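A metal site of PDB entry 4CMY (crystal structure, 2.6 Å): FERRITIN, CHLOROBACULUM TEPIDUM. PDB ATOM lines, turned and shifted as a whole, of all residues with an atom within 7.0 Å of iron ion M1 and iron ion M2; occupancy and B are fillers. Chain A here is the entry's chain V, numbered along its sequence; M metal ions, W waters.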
ATOM      1  N   GLN A  13       7.105  32.503  20.729  1.00  0.00           N
ATOM      2  CA  GLN A  13       6.032  32.256  21.698  1.00  0.00           C
ATOM      3  C   GLN A  13       4.757  33.022  21.345  1.00  0.00           C
ATOM      4  O   GLN A  13       3.665  32.468  21.411  1.00  0.00           O
ATOM      5  CB  GLN A  13       6.480  32.655  23.094  1.00  0.00           C
ATOM      6  CG  GLN A  13       5.637  32.076  24.175  1.00  0.00           C
ATOM      7  CD  GLN A  13       5.729  30.558  24.236  1.00  0.00           C
ATOM      8  OE1 GLN A  13       6.773  29.981  23.995  1.00  0.00           O
ATOM      9  NE2 GLN A  13       4.620  29.908  24.567  1.00  0.00           N
ATOM     10  N   PHE A  16       3.292  30.885  18.804  1.00  0.00           N
ATOM     11  CA  PHE A  16       2.785  29.630  19.416  1.00  0.00           C
ATOM     12  C   PHE A  16       1.428  29.867  20.079  1.00  0.00           C
ATOM     13  O   PHE A  16       0.527  29.056  19.977  1.00  0.00           O
ATOM     14  CB  PHE A  16       3.829  29.144  20.453  1.00  0.00           C
ATOM     15  CG  PHE A  16       3.803  27.651  20.755  1.00  0.00           C
ATOM     16  CD1 PHE A  16       2.919  26.779  20.175  1.00  0.00           C
ATOM     17  CD2 PHE A  16       4.748  27.129  21.612  1.00  0.00           C
ATOM     18  CE1 PHE A  16       2.962  25.427  20.446  1.00  0.00           C
ATOM     19  CE2 PHE A  16       4.784  25.783  21.906  1.00  0.00           C
ATOM     20  CZ  PHE A  16       3.906  24.923  21.320  1.00  0.00           C
ATOM     21  N   GLU A  17       1.292  30.974  20.822  1.00  0.00           N
ATOM     22  CA  GLU A  17       0.030  31.276  21.490  1.00  0.00           C
ATOM     23  C   GLU A  17      -1.043  31.540  20.433  1.00  0.00           C
ATOM     24  O   GLU A  17      -2.165  31.064  20.570  1.00  0.00           O
ATOM     25  CB  GLU A  17       0.170  32.461  22.459  1.00  0.00           C
ATOM     26  CG  GLU A  17       1.186  32.257  23.558  1.00  0.00           C
ATOM     27  CD  GLU A  17       0.810  31.223  24.652  1.00  0.00           C
ATOM     28  OE1 GLU A  17      -0.397  30.926  24.845  1.00  0.00           O
ATOM     29  OE2 GLU A  17       1.749  30.795  25.374  1.00  0.00           O
ATOM     30  N   SER A  20      -2.227  28.347  19.195  1.00  0.00           N
ATOM     31  CA  SER A  20      -3.075  27.660  20.193  1.00  0.00           C
ATOM     32  C   SER A  20      -4.496  28.137  20.124  1.00  0.00           C
ATOM     33  O   SER A  20      -5.411  27.358  20.193  1.00  0.00           O
ATOM     34  CB  SER A  20      -2.546  27.898  21.601  1.00  0.00           C
ATOM     35  OG  SER A  20      -1.173  27.521  21.661  1.00  0.00           O
ATOM     36  N   TYR A  24      -7.601  25.668  19.195  1.00  0.00           N
ATOM     37  CA  TYR A  24      -8.751  25.443  20.072  1.00  0.00           C
ATOM     38  C   TYR A  24     -10.042  25.863  19.412  1.00  0.00           C
ATOM     39  O   TYR A  24     -11.067  25.258  19.623  1.00  0.00           O
ATOM     40  CB  TYR A  24      -8.535  26.140  21.430  1.00  0.00           C
ATOM     41  CG  TYR A  24      -7.389  25.559  22.280  1.00  0.00           C
ATOM     42  CD1 TYR A  24      -6.958  24.255  22.134  1.00  0.00           C
ATOM     43  CD2 TYR A  24      -6.756  26.332  23.253  1.00  0.00           C
ATOM     44  CE1 TYR A  24      -5.927  23.754  22.897  1.00  0.00           C
ATOM     45  CE2 TYR A  24      -5.741  25.842  24.004  1.00  0.00           C
ATOM     46  CZ  TYR A  24      -5.319  24.553  23.825  1.00  0.00           C
ATOM     47  OH  TYR A  24      -4.274  24.028  24.554  1.00  0.00           O
ATOM     48  N   HIS A  46     -11.653  29.065  25.637  1.00  0.00           N
ATOM     49  CA  HIS A  46     -10.252  28.980  25.908  1.00  0.00           C
ATOM     50  C   HIS A  46      -9.397  29.539  24.766  1.00  0.00           C
ATOM     51  O   HIS A  46      -8.262  29.956  24.984  1.00  0.00           O
ATOM     52  CB  HIS A  46      -9.833  27.556  26.231  1.00  0.00           C
ATOM     53  CG  HIS A  46      -8.701  27.520  27.157  1.00  0.00           C
ATOM     54  ND1 HIS A  46      -8.856  27.754  28.504  1.00  0.00           N
ATOM     55  CD2 HIS A  46      -7.366  27.421  26.941  1.00  0.00           C
ATOM     56  CE1 HIS A  46      -7.680  27.767  29.084  1.00  0.00           C
ATOM     57  NE2 HIS A  46      -6.762  27.562  28.164  1.00  0.00           N
ATOM     58  N   GLU A  49      -8.659  32.898  25.784  1.00  0.00           N
ATOM     59  CA  GLU A  49      -7.579  32.952  26.764  1.00  0.00           C
ATOM     60  C   GLU A  49      -6.227  32.911  26.083  1.00  0.00           C
ATOM     61  O   GLU A  49      -5.330  33.653  26.469  1.00  0.00           O
ATOM     62  CB  GLU A  49      -7.676  31.804  27.772  1.00  0.00           C
ATOM     63  CG  GLU A  49      -8.736  32.018  28.838  1.00  0.00           C
ATOM     64  CD  GLU A  49      -8.309  33.069  29.847  1.00  0.00           C
ATOM     65  OE1 GLU A  49      -7.114  33.127  30.290  1.00  0.00           O
ATOM     66  OE2 GLU A  49      -9.201  33.886  30.155  1.00  0.00           O
ATOM     67  N   GLU A  50      -6.079  32.085  25.056  1.00  0.00           N
ATOM     68  CA  GLU A  50      -4.810  32.009  24.374  1.00  0.00           C
ATOM     69  C   GLU A  50      -4.503  33.305  23.643  1.00  0.00           C
ATOM     70  O   GLU A  50      -3.354  33.687  23.525  1.00  0.00           O
ATOM     71  CB  GLU A  50      -4.776  30.788  23.432  1.00  0.00           C
ATOM     72  CG  GLU A  50      -4.909  29.432  24.158  1.00  0.00           C
ATOM     73  CD  GLU A  50      -3.757  29.076  25.116  1.00  0.00           C
ATOM     74  OE1 GLU A  50      -2.707  29.782  25.100  1.00  0.00           O
ATOM     75  OE2 GLU A  50      -3.956  28.076  25.940  1.00  0.00           O
ATOM     76  N   LYS A  51      -5.517  33.985  23.153  1.00  0.00           N
ATOM     77  CA  LYS A  51      -5.354  35.278  22.509  1.00  0.00           C
ATOM     78  C   LYS A  51      -4.848  36.278  23.484  1.00  0.00           C
ATOM     79  O   LYS A  51      -3.981  37.048  23.151  1.00  0.00           O
ATOM     80  CB  LYS A  51      -6.680  35.772  21.942  1.00  0.00           C
ATOM     81  CG  LYS A  51      -6.672  36.256  20.507  1.00  0.00           C
ATOM     82  CD  LYS A  51      -7.222  35.127  19.628  1.00  0.00           C
ATOM     83  CE  LYS A  51      -6.930  35.209  18.132  1.00  0.00           C
ATOM     84  NZ  LYS A  51      -6.920  33.927  17.361  1.00  0.00           N
ATOM     85  N   HIS A  53      -2.970  35.534  26.074  1.00  0.00           N
ATOM     86  CA  HIS A  53      -1.583  35.178  26.315  1.00  0.00           C
ATOM     87  C   HIS A  53      -0.728  35.770  25.222  1.00  0.00           C
ATOM     88  O   HIS A  53       0.354  36.279  25.480  1.00  0.00           O
ATOM     89  CB  HIS A  53      -1.359  33.674  26.335  1.00  0.00           C
ATOM     90  CG  HIS A  53      -2.072  32.956  27.436  1.00  0.00           C
ATOM     91  ND1 HIS A  53      -2.151  31.572  27.493  1.00  0.00           N
ATOM     92  CD2 HIS A  53      -2.800  33.414  28.486  1.00  0.00           C
ATOM     93  CE1 HIS A  53      -2.881  31.217  28.547  1.00  0.00           C
ATOM     94  NE2 HIS A  53      -3.291  32.312  29.159  1.00  0.00           N
ATOM     95  N   MET A  54      -1.206  35.666  23.998  1.00  0.00           N
ATOM     96  CA  MET A  54      -0.484  36.197  22.866  1.00  0.00           C
ATOM     97  C   MET A  54      -0.272  37.682  23.033  1.00  0.00           C
ATOM     98  O   MET A  54       0.836  38.182  22.807  1.00  0.00           O
ATOM     99  CB  MET A  54      -1.230  35.878  21.572  1.00  0.00           C
ATOM    100  CG  MET A  54      -0.572  36.455  20.323  1.00  0.00           C
ATOM    101  SD  MET A  54      -1.628  36.339  18.872  1.00  0.00           S
ATOM    102  CE  MET A  54      -2.721  37.709  19.210  1.00  0.00           C
ATOM    103  N   HIS A  93      -0.328  19.440  23.744  1.00  0.00           N
ATOM    104  CA  HIS A  93      -0.061  20.765  23.243  1.00  0.00           C
ATOM    105  C   HIS A  93       0.259  21.704  24.405  1.00  0.00           C
ATOM    106  O   HIS A  93       1.217  22.485  24.335  1.00  0.00           O
ATOM    107  CB  HIS A  93      -1.250  21.267  22.433  1.00  0.00           C
ATOM    108  CG  HIS A  93      -1.052  22.619  21.875  1.00  0.00           C
ATOM    109  ND1 HIS A  93      -0.428  22.842  20.670  1.00  0.00           N
ATOM    110  CD2 HIS A  93      -1.407  23.844  22.334  1.00  0.00           C
ATOM    111  CE1 HIS A  93      -0.425  24.135  20.401  1.00  0.00           C
ATOM    112  NE2 HIS A  93      -0.995  24.770  21.414  1.00  0.00           N
ATOM    113  N   GLU A  94      -0.514  21.618  25.477  1.00  0.00           N
ATOM    114  CA  GLU A  94      -0.243  22.440  26.651  1.00  0.00           C
ATOM    115  C   GLU A  94       1.086  22.074  27.303  1.00  0.00           C
ATOM    116  O   GLU A  94       1.807  22.969  27.753  1.00  0.00           O
ATOM    117  CB  GLU A  94      -1.406  22.416  27.655  1.00  0.00           C
ATOM    118  CG  GLU A  94      -2.633  23.243  27.194  1.00  0.00           C
ATOM    119  CD  GLU A  94      -2.429  24.749  27.236  1.00  0.00           C
ATOM    120  OE1 GLU A  94      -1.481  25.152  27.965  1.00  0.00           O
ATOM    121  OE2 GLU A  94      -3.208  25.529  26.584  1.00  0.00           O
ATOM    122  N   ILE A  97       3.679  23.824  25.273  1.00  0.00           N
ATOM    123  CA  ILE A  97       3.723  25.250  25.562  1.00  0.00           C
ATOM    124  C   ILE A  97       4.525  25.433  26.837  1.00  0.00           C
ATOM    125  O   ILE A  97       5.384  26.318  26.904  1.00  0.00           O
ATOM    126  CB  ILE A  97       2.311  25.864  25.709  1.00  0.00           C
ATOM    127  CG1 ILE A  97       1.685  25.989  24.344  1.00  0.00           C
ATOM    128  CG2 ILE A  97       2.391  27.274  26.287  1.00  0.00           C
ATOM    129  CD1 ILE A  97       0.214  26.216  24.424  1.00  0.00           C
ATOM    130  N   ILE A 101       7.876  27.728  27.365  1.00  0.00           N
ATOM    131  CA  ILE A 101       7.991  28.772  28.376  1.00  0.00           C
ATOM    132  C   ILE A 101       9.207  28.492  29.272  1.00  0.00           C
ATOM    133  O   ILE A 101       9.976  29.396  29.562  1.00  0.00           O
ATOM    134  CB  ILE A 101       6.722  28.878  29.242  1.00  0.00           C
ATOM    135  CG1 ILE A 101       5.527  29.358  28.436  1.00  0.00           C
ATOM    136  CG2 ILE A 101       6.965  29.811  30.415  1.00  0.00           C
ATOM    137  CD1 ILE A 101       5.631  30.772  27.901  1.00  0.00           C
ATOM    138  N   TRP A 122       4.495  35.142  35.245  1.00  0.00           N
ATOM    139  CA  TRP A 122       3.083  35.070  34.999  1.00  0.00           C
ATOM    140  C   TRP A 122       2.733  33.831  34.170  1.00  0.00           C
ATOM    141  O   TRP A 122       1.806  33.107  34.514  1.00  0.00           O
ATOM    142  CB  TRP A 122       2.613  36.324  34.278  1.00  0.00           C
ATOM    143  CG  TRP A 122       1.152  36.366  34.190  1.00  0.00           C
ATOM    144  CD1 TRP A 122       0.314  36.900  35.116  1.00  0.00           C
ATOM    145  CD2 TRP A 122       0.324  35.831  33.131  1.00  0.00           C
ATOM    146  NE1 TRP A 122      -1.002  36.761  34.695  1.00  0.00           N
ATOM    147  CE2 TRP A 122      -1.022  36.100  33.483  1.00  0.00           C
ATOM    148  CE3 TRP A 122       0.581  35.183  31.926  1.00  0.00           C
ATOM    149  CZ2 TRP A 122      -2.110  35.731  32.688  1.00  0.00           C
ATOM    150  CZ3 TRP A 122      -0.486  34.816  31.123  1.00  0.00           C
ATOM    151  CH2 TRP A 122      -1.824  35.090  31.511  1.00  0.00           C
ATOM    152  N   TYR A 123       3.490  33.582  33.095  1.00  0.00           N
ATOM    153  CA  TYR A 123       3.261  32.416  32.227  1.00  0.00           C
ATOM    154  C   TYR A 123       3.570  31.099  32.912  1.00  0.00           C
ATOM    155  O   TYR A 123       2.916  30.093  32.663  1.00  0.00           O
ATOM    156  CB  TYR A 123       4.079  32.495  30.908  1.00  0.00           C
ATOM    157  CG  TYR A 123       3.528  33.533  29.998  1.00  0.00           C
ATOM    158  CD1 TYR A 123       3.877  34.852  30.173  1.00  0.00           C
ATOM    159  CD2 TYR A 123       2.619  33.224  29.024  1.00  0.00           C
ATOM    160  CE1 TYR A 123       3.319  35.858  29.387  1.00  0.00           C
ATOM    161  CE2 TYR A 123       2.076  34.213  28.220  1.00  0.00           C
ATOM    162  CZ  TYR A 123       2.427  35.527  28.423  1.00  0.00           C
ATOM    163  OH  TYR A 123       1.912  36.532  27.663  1.00  0.00           O
ATOM    164  N   GLU A 126       0.619  30.506  34.959  1.00  0.00           N
ATOM    165  CA  GLU A 126      -0.560  30.237  34.144  1.00  0.00           C
ATOM    166  C   GLU A 126      -0.500  28.838  33.545  1.00  0.00           C
ATOM    167  O   GLU A 126      -1.490  28.156  33.497  1.00  0.00           O
ATOM    168  CB  GLU A 126      -0.710  31.277  33.039  1.00  0.00           C
ATOM    169  CG  GLU A 126      -2.054  31.219  32.310  1.00  0.00           C
ATOM    170  CD  GLU A 126      -3.258  31.743  33.119  1.00  0.00           C
ATOM    171  OE1 GLU A 126      -3.085  32.351  34.214  1.00  0.00           O
ATOM    172  OE2 GLU A 126      -4.400  31.551  32.587  1.00  0.00           O
ATOM    173  N   GLN A 127       0.686  28.382  33.171  1.00  0.00           N
ATOM    174  CA  GLN A 127       0.816  27.051  32.608  1.00  0.00           C
ATOM    175  C   GLN A 127       0.589  25.955  33.632  1.00  0.00           C
ATOM    176  O   GLN A 127       0.140  24.864  33.278  1.00  0.00           O
ATOM    177  CB  GLN A 127       2.146  26.865  31.876  1.00  0.00           C
ATOM    178  CG  GLN A 127       2.121  27.651  30.571  1.00  0.00           C
ATOM    179  CD  GLN A 127       1.076  27.159  29.610  1.00  0.00           C
ATOM    180  OE1 GLN A 127       0.280  27.951  29.069  1.00  0.00           O
ATOM    181  NE2 GLN A 127       1.037  25.842  29.404  1.00  0.00           N
ATOM    182  N   GLU A 130      -3.062  25.693  33.485  1.00  0.00           N
ATOM    183  CA  GLU A 130      -3.470  25.082  32.217  1.00  0.00           C
ATOM    184  C   GLU A 130      -3.295  23.583  32.248  1.00  0.00           C
ATOM    185  O   GLU A 130      -4.158  22.839  31.824  1.00  0.00           O
ATOM    186  CB  GLU A 130      -2.651  25.625  31.039  1.00  0.00           C
ATOM    187  CG  GLU A 130      -2.831  27.090  30.723  1.00  0.00           C
ATOM    188  CD  GLU A 130      -4.050  27.352  29.875  1.00  0.00           C
ATOM    189  OE1 GLU A 130      -3.938  27.288  28.594  1.00  0.00           O
ATOM    190  OE2 GLU A 130      -5.106  27.610  30.502  1.00  0.00           O
ATOM    191  N   PHE A 134      -6.391  20.880  31.811  1.00  0.00           N
ATOM    192  CA  PHE A 134      -6.432  19.937  30.697  1.00  0.00           C
ATOM    193  C   PHE A 134      -6.164  18.493  31.098  1.00  0.00           C
ATOM    194  O   PHE A 134      -6.762  17.589  30.553  1.00  0.00           O
ATOM    195  CB  PHE A 134      -5.499  20.378  29.560  1.00  0.00           C
ATOM    196  CG  PHE A 134      -6.032  21.525  28.731  1.00  0.00           C
ATOM    197  CD1 PHE A 134      -6.829  21.288  27.655  1.00  0.00           C
ATOM    198  CD2 PHE A 134      -5.731  22.834  29.065  1.00  0.00           C
ATOM    199  CE1 PHE A 134      -7.330  22.331  26.915  1.00  0.00           C
ATOM    200  CE2 PHE A 134      -6.239  23.883  28.348  1.00  0.00           C
ATOM    201  CZ  PHE A 134      -7.042  23.637  27.263  1.00  0.00           C
HETATM  202 FE    FE M   1      -2.567  27.475  27.103  1.00  0.00          FE
HETATM  203 FE    FE M   2      -1.123  29.930  26.518  1.00  0.00          FE
HETATM  204  O   HOH W   1       0.823  30.467  27.965  1.00  0.00           O
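The side-chain hydroxyl of Tyr 123 sits at hydrogen-bond distance from the backbone carbonyl oxygen of His 53, at 2.7 Å.
The side-chain amide nitrogen of Gln 127 sits at hydrogen-bond distance from the side-chain carboxylate of Glu 94, at 3.0 Å.
The side-chain carboxylate of Glu 17 sits at hydrogen-bond distance from the side-chain amide nitrogen of Gln 13 (3.1 Å).
A ring nitrogen (NE2) of His 46 lies within hydrogen-bond range of the side-chain carboxylate (OE2) of Glu 130 (2.9 Å).
The side-chain hydroxyl of Tyr 24 lies close to the side-chain carboxylate of Glu 94, 2.7 Å away.
Residues that only touch iron ion M1: Gln 127.
Residues that only touch iron ion M2: Gln 127 (3.5 Å).
Of the 21 residues printed, 4 come within 4 Å of iron ion M2.
The nearest printed residue that does not touch iron ion M2 is Glu 130 (4.4 Å).
Iron ion M1 is bound by the side-chain carboxylate (OE2) of Glu 50, the side-chain carboxylate (OE1) of Glu 130 and the side-chain carboxylate (OE2) of Glu 94.
Iron ion M1 has three donor atoms within binding distance.
Slightly farther from iron ion M1 lies the side-chain carboxylate (OE1) of Glu 94 (2.7 Å).
Iron ion M2 is bound by the side-chain carboxylate of Glu 17, the side-chain carboxylate of Glu 50, a ring nitrogen (ND1) of His 53 and water W1.
Water W1 lies within hydrogen-bond range of OE2 of Glu 17 and OE1 of Gln 127.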
